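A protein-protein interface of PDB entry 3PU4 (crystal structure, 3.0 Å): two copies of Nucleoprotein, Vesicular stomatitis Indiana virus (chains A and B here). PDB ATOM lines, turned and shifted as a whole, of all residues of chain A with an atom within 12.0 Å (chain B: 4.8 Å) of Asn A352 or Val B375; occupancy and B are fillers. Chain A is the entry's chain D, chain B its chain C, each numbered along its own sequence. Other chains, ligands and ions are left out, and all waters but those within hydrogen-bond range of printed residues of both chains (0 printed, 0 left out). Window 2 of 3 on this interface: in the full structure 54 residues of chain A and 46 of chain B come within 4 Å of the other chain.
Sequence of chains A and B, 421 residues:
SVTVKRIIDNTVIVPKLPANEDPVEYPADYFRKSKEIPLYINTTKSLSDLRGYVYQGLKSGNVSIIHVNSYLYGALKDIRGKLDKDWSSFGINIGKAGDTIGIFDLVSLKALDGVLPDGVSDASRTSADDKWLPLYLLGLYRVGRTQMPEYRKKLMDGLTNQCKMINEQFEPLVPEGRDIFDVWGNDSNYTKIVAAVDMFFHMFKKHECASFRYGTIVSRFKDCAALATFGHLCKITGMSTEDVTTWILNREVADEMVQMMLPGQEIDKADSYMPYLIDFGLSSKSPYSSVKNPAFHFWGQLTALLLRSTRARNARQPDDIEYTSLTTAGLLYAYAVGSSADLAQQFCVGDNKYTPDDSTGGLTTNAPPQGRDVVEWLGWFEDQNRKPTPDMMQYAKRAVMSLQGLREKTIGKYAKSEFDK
NZ of Lys A353 lies close to N of Gly B379 (3.3 Å).
OD1 of Asp B373 is in hydrogen-bond range of N of Val B375, 2.8 Å away.
The side-chain amide oxygen of Gln A345 sits at hydrogen-bond distance from the backbone NH of Lys A353 (2.9 Å).
The side-chain amide nitrogen (NE2) of Gln A345 sits at hydrogen-bond distance from the backbone carbonyl oxygen (O) of Phe A347 (2.7 Å).
Among the printed residues, pairs that only touch across the chains: Gln A345 with Val B374 (3.8 Å), Gln A345 with Leu B378 (3.3 Å), Asp A351 with Val B375 (3.3 Å), Asn A352 with Val B375 (3.4 Å), Lys A353 with Val B375 (3.2 Å) and Lys A353 with Leu B378 (3.7 Å).
Of the printed residues of chain A, Val B375 touches Asp A351 (3.3 Å), Asn A352 (3.4 Å) and Lys A353 (3.2 Å).
No residue of chain A comes within 4 Å of Asp B373.
Val B374 touches just one residue of chain A: Gln A345 (3.8 Å).
No residue of chain A comes within 4 Å of Glu B376.
Of chain A, only Gln A345 and Lys A353 come within 4 Å of Leu B378.
Gly B379 touches just one residue of chain A: Lys A353.
Of the printed residues of chain B, Gln A345 touches Val B374 and Leu B378.
Printed residues of chain B within 4 Å of Lys A353: Val B375 (3.2 Å), Leu B378 (3.7 Å) and Gly B379 (3.0 Å).
Asp A357 touches none of the printed residues of chain B.
The nearest printed residue of chain B that does not touch Lys A353 is Val B374 (5.5 Å).
Printed residues of chain A that touch a printed residue of chain B: Gln A345, Asp A351, Asn A352 and Lys A353.
Of the 7 printed residues of chain B, 4 touch a printed residue of chain A.
Among the printed residues, no Asp or Glu carboxylate lies within 4 Å of a Lys or Arg side-chain nitrogen of the other chain.
No position is printed for both chains.
Of the 7 pairs that touch across the chains among the printed residues, none has its exchanged pair printed and touching as well.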
ATOM      1  N   LEU A 343      -8.997 -19.809 -11.929  1.00  0.00           N
ATOM      2  CA  LEU A 343      -9.251 -21.044 -11.201  1.00  0.00           C
ATOM      3  C   LEU A 343      -8.488 -21.178  -9.883  1.00  0.00           C
ATOM      4  O   LEU A 343      -7.315 -21.576  -9.860  1.00  0.00           O
ATOM      5  CB  LEU A 343      -8.951 -22.238 -12.107  1.00  0.00           C
ATOM      6  CG  LEU A 343     -10.234 -22.930 -12.545  1.00  0.00           C
ATOM      7  CD1 LEU A 343     -11.016 -23.334 -11.308  1.00  0.00           C
ATOM      8  CD2 LEU A 343     -11.075 -22.009 -13.399  1.00  0.00           C
ATOM      9  N   ALA A 344      -9.161 -20.873  -8.780  1.00  0.00           N
ATOM     10  CA  ALA A 344      -8.560 -21.026  -7.443  1.00  0.00           C
ATOM     11  C   ALA A 344      -9.633 -21.189  -6.371  1.00  0.00           C
ATOM     12  O   ALA A 344     -10.552 -20.386  -6.288  1.00  0.00           O
ATOM     13  CB  ALA A 344      -7.676 -19.837  -7.119  1.00  0.00           C
ATOM     14  N   GLN A 345      -9.527 -22.228  -5.558  1.00  0.00           N
ATOM     15  CA  GLN A 345     -10.559 -22.466  -4.572  1.00  0.00           C
ATOM     16  C   GLN A 345     -10.753 -21.182  -3.791  1.00  0.00           C
ATOM     17  O   GLN A 345      -9.766 -20.520  -3.477  1.00  0.00           O
ATOM     18  CB  GLN A 345     -10.184 -23.609  -3.638  1.00  0.00           C
ATOM     19  CG  GLN A 345     -11.379 -24.089  -2.841  1.00  0.00           C
ATOM     20  CD  GLN A 345     -11.019 -24.999  -1.712  1.00  0.00           C
ATOM     21  OE1 GLN A 345      -9.957 -25.590  -1.708  1.00  0.00           O
ATOM     22  NE2 GLN A 345     -11.905 -25.121  -0.743  1.00  0.00           N
ATOM     23  N   GLN A 346     -12.009 -20.834  -3.480  1.00  0.00           N
ATOM     24  CA  GLN A 346     -12.315 -19.553  -2.852  1.00  0.00           C
ATOM     25  C   GLN A 346     -12.939 -19.655  -1.458  1.00  0.00           C
ATOM     26  O   GLN A 346     -12.635 -18.848  -0.596  1.00  0.00           O
ATOM     27  CB  GLN A 346     -13.207 -18.732  -3.773  1.00  0.00           C
ATOM     28  CG  GLN A 346     -12.652 -18.533  -5.157  1.00  0.00           C
ATOM     29  CD  GLN A 346     -11.707 -17.362  -5.239  1.00  0.00           C
ATOM     30  OE1 GLN A 346     -10.775 -17.372  -6.037  1.00  0.00           O
ATOM     31  NE2 GLN A 346     -11.941 -16.343  -4.425  1.00  0.00           N
ATOM     32  N   PHE A 347     -13.830 -20.616  -1.240  1.00  0.00           N
ATOM     33  CA  PHE A 347     -14.395 -20.845   0.099  1.00  0.00           C
ATOM     34  C   PHE A 347     -14.040 -22.262   0.575  1.00  0.00           C
ATOM     35  O   PHE A 347     -13.687 -23.112  -0.242  1.00  0.00           O
ATOM     36  CB  PHE A 347     -15.921 -20.664   0.095  1.00  0.00           C
ATOM     37  CG  PHE A 347     -16.370 -19.319  -0.386  1.00  0.00           C
ATOM     38  CD1 PHE A 347     -16.630 -19.109  -1.724  1.00  0.00           C
ATOM     39  CD2 PHE A 347     -16.535 -18.272   0.494  1.00  0.00           C
ATOM     40  CE1 PHE A 347     -17.038 -17.862  -2.178  1.00  0.00           C
ATOM     41  CE2 PHE A 347     -16.928 -17.041   0.062  1.00  0.00           C
ATOM     42  CZ  PHE A 347     -17.185 -16.826  -1.273  1.00  0.00           C
ATOM     43  N   CYS A 348     -14.139 -22.533   1.877  1.00  0.00           N
ATOM     44  CA  CYS A 348     -13.822 -23.873   2.364  1.00  0.00           C
ATOM     45  C   CYS A 348     -14.469 -24.264   3.689  1.00  0.00           C
ATOM     46  O   CYS A 348     -15.093 -23.450   4.342  1.00  0.00           O
ATOM     47  CB  CYS A 348     -12.313 -24.012   2.501  1.00  0.00           C
ATOM     48  SG  CYS A 348     -11.589 -23.098   3.894  1.00  0.00           S
ATOM     49  N   VAL A 349     -14.288 -25.520   4.083  1.00  0.00           N
ATOM     50  CA  VAL A 349     -14.741 -25.990   5.386  1.00  0.00           C
ATOM     51  C   VAL A 349     -13.637 -26.672   6.219  1.00  0.00           C
ATOM     52  O   VAL A 349     -13.828 -27.782   6.703  1.00  0.00           O
ATOM     53  CB  VAL A 349     -15.903 -26.973   5.232  1.00  0.00           C
ATOM     54  CG1 VAL A 349     -16.724 -26.986   6.499  1.00  0.00           C
ATOM     55  CG2 VAL A 349     -16.766 -26.589   4.058  1.00  0.00           C
ATOM     56  N   GLY A 350     -12.493 -26.011   6.395  1.00  0.00           N
ATOM     57  CA  GLY A 350     -11.361 -26.599   7.099  1.00  0.00           C
ATOM     58  C   GLY A 350     -10.344 -27.348   6.230  1.00  0.00           C
ATOM     59  O   GLY A 350      -9.289 -27.756   6.730  1.00  0.00           O
ATOM     60  N   ASP A 351     -10.647 -27.542   4.941  1.00  0.00           N
ATOM     61  CA  ASP A 351      -9.711 -28.216   4.018  1.00  0.00           C
ATOM     62  C   ASP A 351      -9.496 -27.524   2.657  1.00  0.00           C
ATOM     63  O   ASP A 351     -10.225 -27.775   1.703  1.00  0.00           O
ATOM     64  CB  ASP A 351     -10.113 -29.683   3.794  1.00  0.00           C
ATOM     65  CG  ASP A 351     -11.325 -29.838   2.880  1.00  0.00           C
ATOM     66  OD1 ASP A 351     -11.383 -30.815   2.092  1.00  0.00           O
ATOM     67  OD2 ASP A 351     -12.221 -28.976   2.956  1.00  0.00           O
ATOM     68  N   ASN A 352      -8.478 -26.670   2.571  1.00  0.00           N
ATOM     69  CA  ASN A 352      -8.176 -25.966   1.328  1.00  0.00           C
ATOM     70  C   ASN A 352      -7.478 -26.921   0.372  1.00  0.00           C
ATOM     71  O   ASN A 352      -7.105 -28.018   0.773  1.00  0.00           O
ATOM     72  CB  ASN A 352      -7.264 -24.738   1.547  1.00  0.00           C
ATOM     73  CG  ASN A 352      -7.281 -24.202   2.984  1.00  0.00           C
ATOM     74  OD1 ASN A 352      -7.953 -24.734   3.862  1.00  0.00           O
ATOM     75  ND2 ASN A 352      -6.520 -23.137   3.218  1.00  0.00           N
ATOM     76  N   LYS A 353      -7.303 -26.513  -0.887  1.00  0.00           N
ATOM     77  CA  LYS A 353      -6.364 -27.197  -1.774  1.00  0.00           C
ATOM     78  C   LYS A 353      -5.151 -26.319  -1.903  1.00  0.00           C
ATOM     79  O   LYS A 353      -5.257 -25.205  -2.396  1.00  0.00           O
ATOM     80  CB  LYS A 353      -6.944 -27.433  -3.166  1.00  0.00           C
ATOM     81  CG  LYS A 353      -5.945 -28.069  -4.140  1.00  0.00           C
ATOM     82  CD  LYS A 353      -5.594 -27.141  -5.300  1.00  0.00           C
ATOM     83  CE  LYS A 353      -4.442 -27.687  -6.146  1.00  0.00           C
ATOM     84  NZ  LYS A 353      -4.622 -29.103  -6.593  1.00  0.00           N
ATOM     85  N   TYR A 354      -4.005 -26.793  -1.434  1.00  0.00           N
ATOM     86  CA  TYR A 354      -2.771 -26.077  -1.688  1.00  0.00           C
ATOM     87  C   TYR A 354      -2.267 -26.514  -3.043  1.00  0.00           C
ATOM     88  O   TYR A 354      -1.908 -27.672  -3.244  1.00  0.00           O
ATOM     89  CB  TYR A 354      -1.726 -26.349  -0.615  1.00  0.00           C
ATOM     90  CG  TYR A 354      -1.905 -25.526   0.645  1.00  0.00           C
ATOM     91  CD1 TYR A 354      -2.693 -24.371   0.647  1.00  0.00           C
ATOM     92  CD2 TYR A 354      -1.273 -25.894   1.835  1.00  0.00           C
ATOM     93  CE1 TYR A 354      -2.857 -23.611   1.810  1.00  0.00           C
ATOM     94  CE2 TYR A 354      -1.428 -25.145   2.998  1.00  0.00           C
ATOM     95  CZ  TYR A 354      -2.219 -24.006   2.984  1.00  0.00           C
ATOM     96  OH  TYR A 354      -2.362 -23.277   4.149  1.00  0.00           O
ATOM     97  N   THR A 355      -2.254 -25.577  -3.978  1.00  0.00           N
ATOM     98  CA  THR A 355      -1.861 -25.871  -5.344  1.00  0.00           C
ATOM     99  C   THR A 355      -0.586 -26.704  -5.459  1.00  0.00           C
ATOM    100  O   THR A 355      -0.472 -27.504  -6.385  1.00  0.00           O
ATOM    101  CB  THR A 355      -1.680 -24.594  -6.154  1.00  0.00           C
ATOM    102  OG1 THR A 355      -0.310 -24.492  -6.557  1.00  0.00           O
ATOM    103  CG2 THR A 355      -2.073 -23.370  -5.317  1.00  0.00           C
ATOM    104  N   PRO A 356       0.385 -26.507  -4.539  1.00  0.00           N
ATOM    105  CA  PRO A 356       1.597 -27.335  -4.538  1.00  0.00           C
ATOM    106  C   PRO A 356       1.307 -28.713  -5.131  1.00  0.00           C
ATOM    107  O   PRO A 356       0.498 -29.481  -4.611  1.00  0.00           O
ATOM    108  CB  PRO A 356       1.978 -27.377  -3.055  1.00  0.00           C
ATOM    109  CG  PRO A 356       1.500 -26.016  -2.526  1.00  0.00           C
ATOM    110  CD  PRO A 356       0.486 -25.442  -3.528  1.00  0.00           C
ATOM    111  N   ASP A 357       1.898 -28.948  -6.298  1.00  0.00           N
ATOM    112  CA  ASP A 357       1.495 -30.025  -7.199  1.00  0.00           C
ATOM    113  C   ASP A 357       1.026 -31.299  -6.490  1.00  0.00           C
ATOM    114  O   ASP A 357       1.819 -32.020  -5.878  1.00  0.00           O
ATOM    115  CB  ASP A 357       2.629 -30.328  -8.187  1.00  0.00           C
ATOM    116  CG  ASP A 357       2.995 -29.121  -9.060  1.00  0.00           C
ATOM    117  OD1 ASP A 357       4.061 -29.168  -9.725  1.00  0.00           O
ATOM    118  OD2 ASP A 357       2.215 -28.134  -9.082  1.00  0.00           O
ATOM    119  N   ASP B 373     -16.034 -33.240  -4.409  1.00  0.00           N
ATOM    120  CA  ASP B 373     -15.264 -32.403  -3.525  1.00  0.00           C
ATOM    121  C   ASP B 373     -14.319 -31.494  -4.253  1.00  0.00           C
ATOM    122  O   ASP B 373     -13.554 -31.934  -5.098  1.00  0.00           O
ATOM    123  CB  ASP B 373     -14.495 -33.211  -2.509  1.00  0.00           C
ATOM    124  CG  ASP B 373     -13.858 -32.330  -1.479  1.00  0.00           C
ATOM    125  OD1 ASP B 373     -12.688 -31.922  -1.679  1.00  0.00           O
ATOM    126  OD2 ASP B 373     -14.558 -32.003  -0.496  1.00  0.00           O
ATOM    127  N   VAL B 374     -14.368 -30.221  -3.887  1.00  0.00           N
ATOM    128  CA  VAL B 374     -13.624 -29.191  -4.580  1.00  0.00           C
ATOM    129  C   VAL B 374     -12.158 -29.514  -4.579  1.00  0.00           C
ATOM    130  O   VAL B 374     -11.466 -29.367  -5.594  1.00  0.00           O
ATOM    131  CB  VAL B 374     -13.792 -27.832  -3.919  1.00  0.00           C
ATOM    132  CG1 VAL B 374     -13.177 -26.776  -4.797  1.00  0.00           C
ATOM    133  CG2 VAL B 374     -15.267 -27.528  -3.706  1.00  0.00           C
ATOM    134  N   VAL B 375     -11.668 -29.963  -3.438  1.00  0.00           N
ATOM    135  CA  VAL B 375     -10.248 -30.178  -3.347  1.00  0.00           C
ATOM    136  C   VAL B 375      -9.830 -31.359  -4.197  1.00  0.00           C
ATOM    137  O   VAL B 375      -8.826 -31.294  -4.903  1.00  0.00           O
ATOM    138  CB  VAL B 375      -9.805 -30.369  -1.936  1.00  0.00           C
ATOM    139  CG1 VAL B 375      -8.389 -29.888  -1.801  1.00  0.00           C
ATOM    140  CG2 VAL B 375     -10.720 -29.604  -1.007  1.00  0.00           C
ATOM    141  N   GLU B 376     -10.591 -32.439  -4.149  1.00  0.00           N
ATOM    142  CA  GLU B 376     -10.228 -33.576  -4.972  1.00  0.00           C
ATOM    143  C   GLU B 376     -10.184 -33.144  -6.444  1.00  0.00           C
ATOM    144  O   GLU B 376      -9.272 -33.503  -7.194  1.00  0.00           O
ATOM    145  CB  GLU B 376     -11.180 -34.759  -4.761  1.00  0.00           C
ATOM    146  CG  GLU B 376     -11.098 -35.406  -3.375  1.00  0.00           C
ATOM    147  CD  GLU B 376     -11.646 -36.833  -3.347  1.00  0.00           C
ATOM    148  OE1 GLU B 376     -12.456 -37.160  -2.450  1.00  0.00           O
ATOM    149  OE2 GLU B 376     -11.267 -37.632  -4.228  1.00  0.00           O
ATOM    150  N   TRP B 377     -11.153 -32.337  -6.853  1.00  0.00           N
ATOM    151  CA  TRP B 377     -11.275 -32.003  -8.254  1.00  0.00           C
ATOM    152  C   TRP B 377     -10.243 -30.990  -8.696  1.00  0.00           C
ATOM    153  O   TRP B 377      -9.618 -31.144  -9.739  1.00  0.00           O
ATOM    154  CB  TRP B 377     -12.660 -31.507  -8.525  1.00  0.00           C
ATOM    155  CG  TRP B 377     -13.615 -32.590  -8.581  1.00  0.00           C
ATOM    156  CD1 TRP B 377     -14.341 -33.102  -7.549  1.00  0.00           C
ATOM    157  CD2 TRP B 377     -13.981 -33.323  -9.735  1.00  0.00           C
ATOM    158  NE1 TRP B 377     -15.153 -34.113  -7.998  1.00  0.00           N
ATOM    159  CE2 TRP B 377     -14.946 -34.268  -9.340  1.00  0.00           C
ATOM    160  CE3 TRP B 377     -13.598 -33.262 -11.073  1.00  0.00           C
ATOM    161  CZ2 TRP B 377     -15.529 -35.143 -10.227  1.00  0.00           C
ATOM    162  CZ3 TRP B 377     -14.169 -34.133 -11.960  1.00  0.00           C
ATOM    163  CH2 TRP B 377     -15.130 -35.065 -11.537  1.00  0.00           C
ATOM    164  N   LEU B 378     -10.064 -29.945  -7.906  1.00  0.00           N
ATOM    165  CA  LEU B 378      -9.056 -28.953  -8.228  1.00  0.00           C
ATOM    166  C   LEU B 378      -7.743 -29.666  -8.518  1.00  0.00           C
ATOM    167  O   LEU B 378      -7.089 -29.410  -9.538  1.00  0.00           O
ATOM    168  CB  LEU B 378      -8.887 -27.971  -7.074  1.00  0.00           C
ATOM    169  CG  LEU B 378      -9.733 -26.720  -7.241  1.00  0.00           C
ATOM    170  CD1 LEU B 378      -9.689 -25.856  -5.985  1.00  0.00           C
ATOM    171  CD2 LEU B 378      -9.237 -25.979  -8.448  1.00  0.00           C
ATOM    172  N   GLY B 379      -7.372 -30.574  -7.612  1.00  0.00           N
ATOM    173  CA  GLY B 379      -6.181 -31.377  -7.759  1.00  0.00           C
ATOM    174  C   GLY B 379      -6.217 -32.205  -9.026  1.00  0.00           C
ATOM    175  O   GLY B 379      -5.278 -32.173  -9.817  1.00  0.00           O
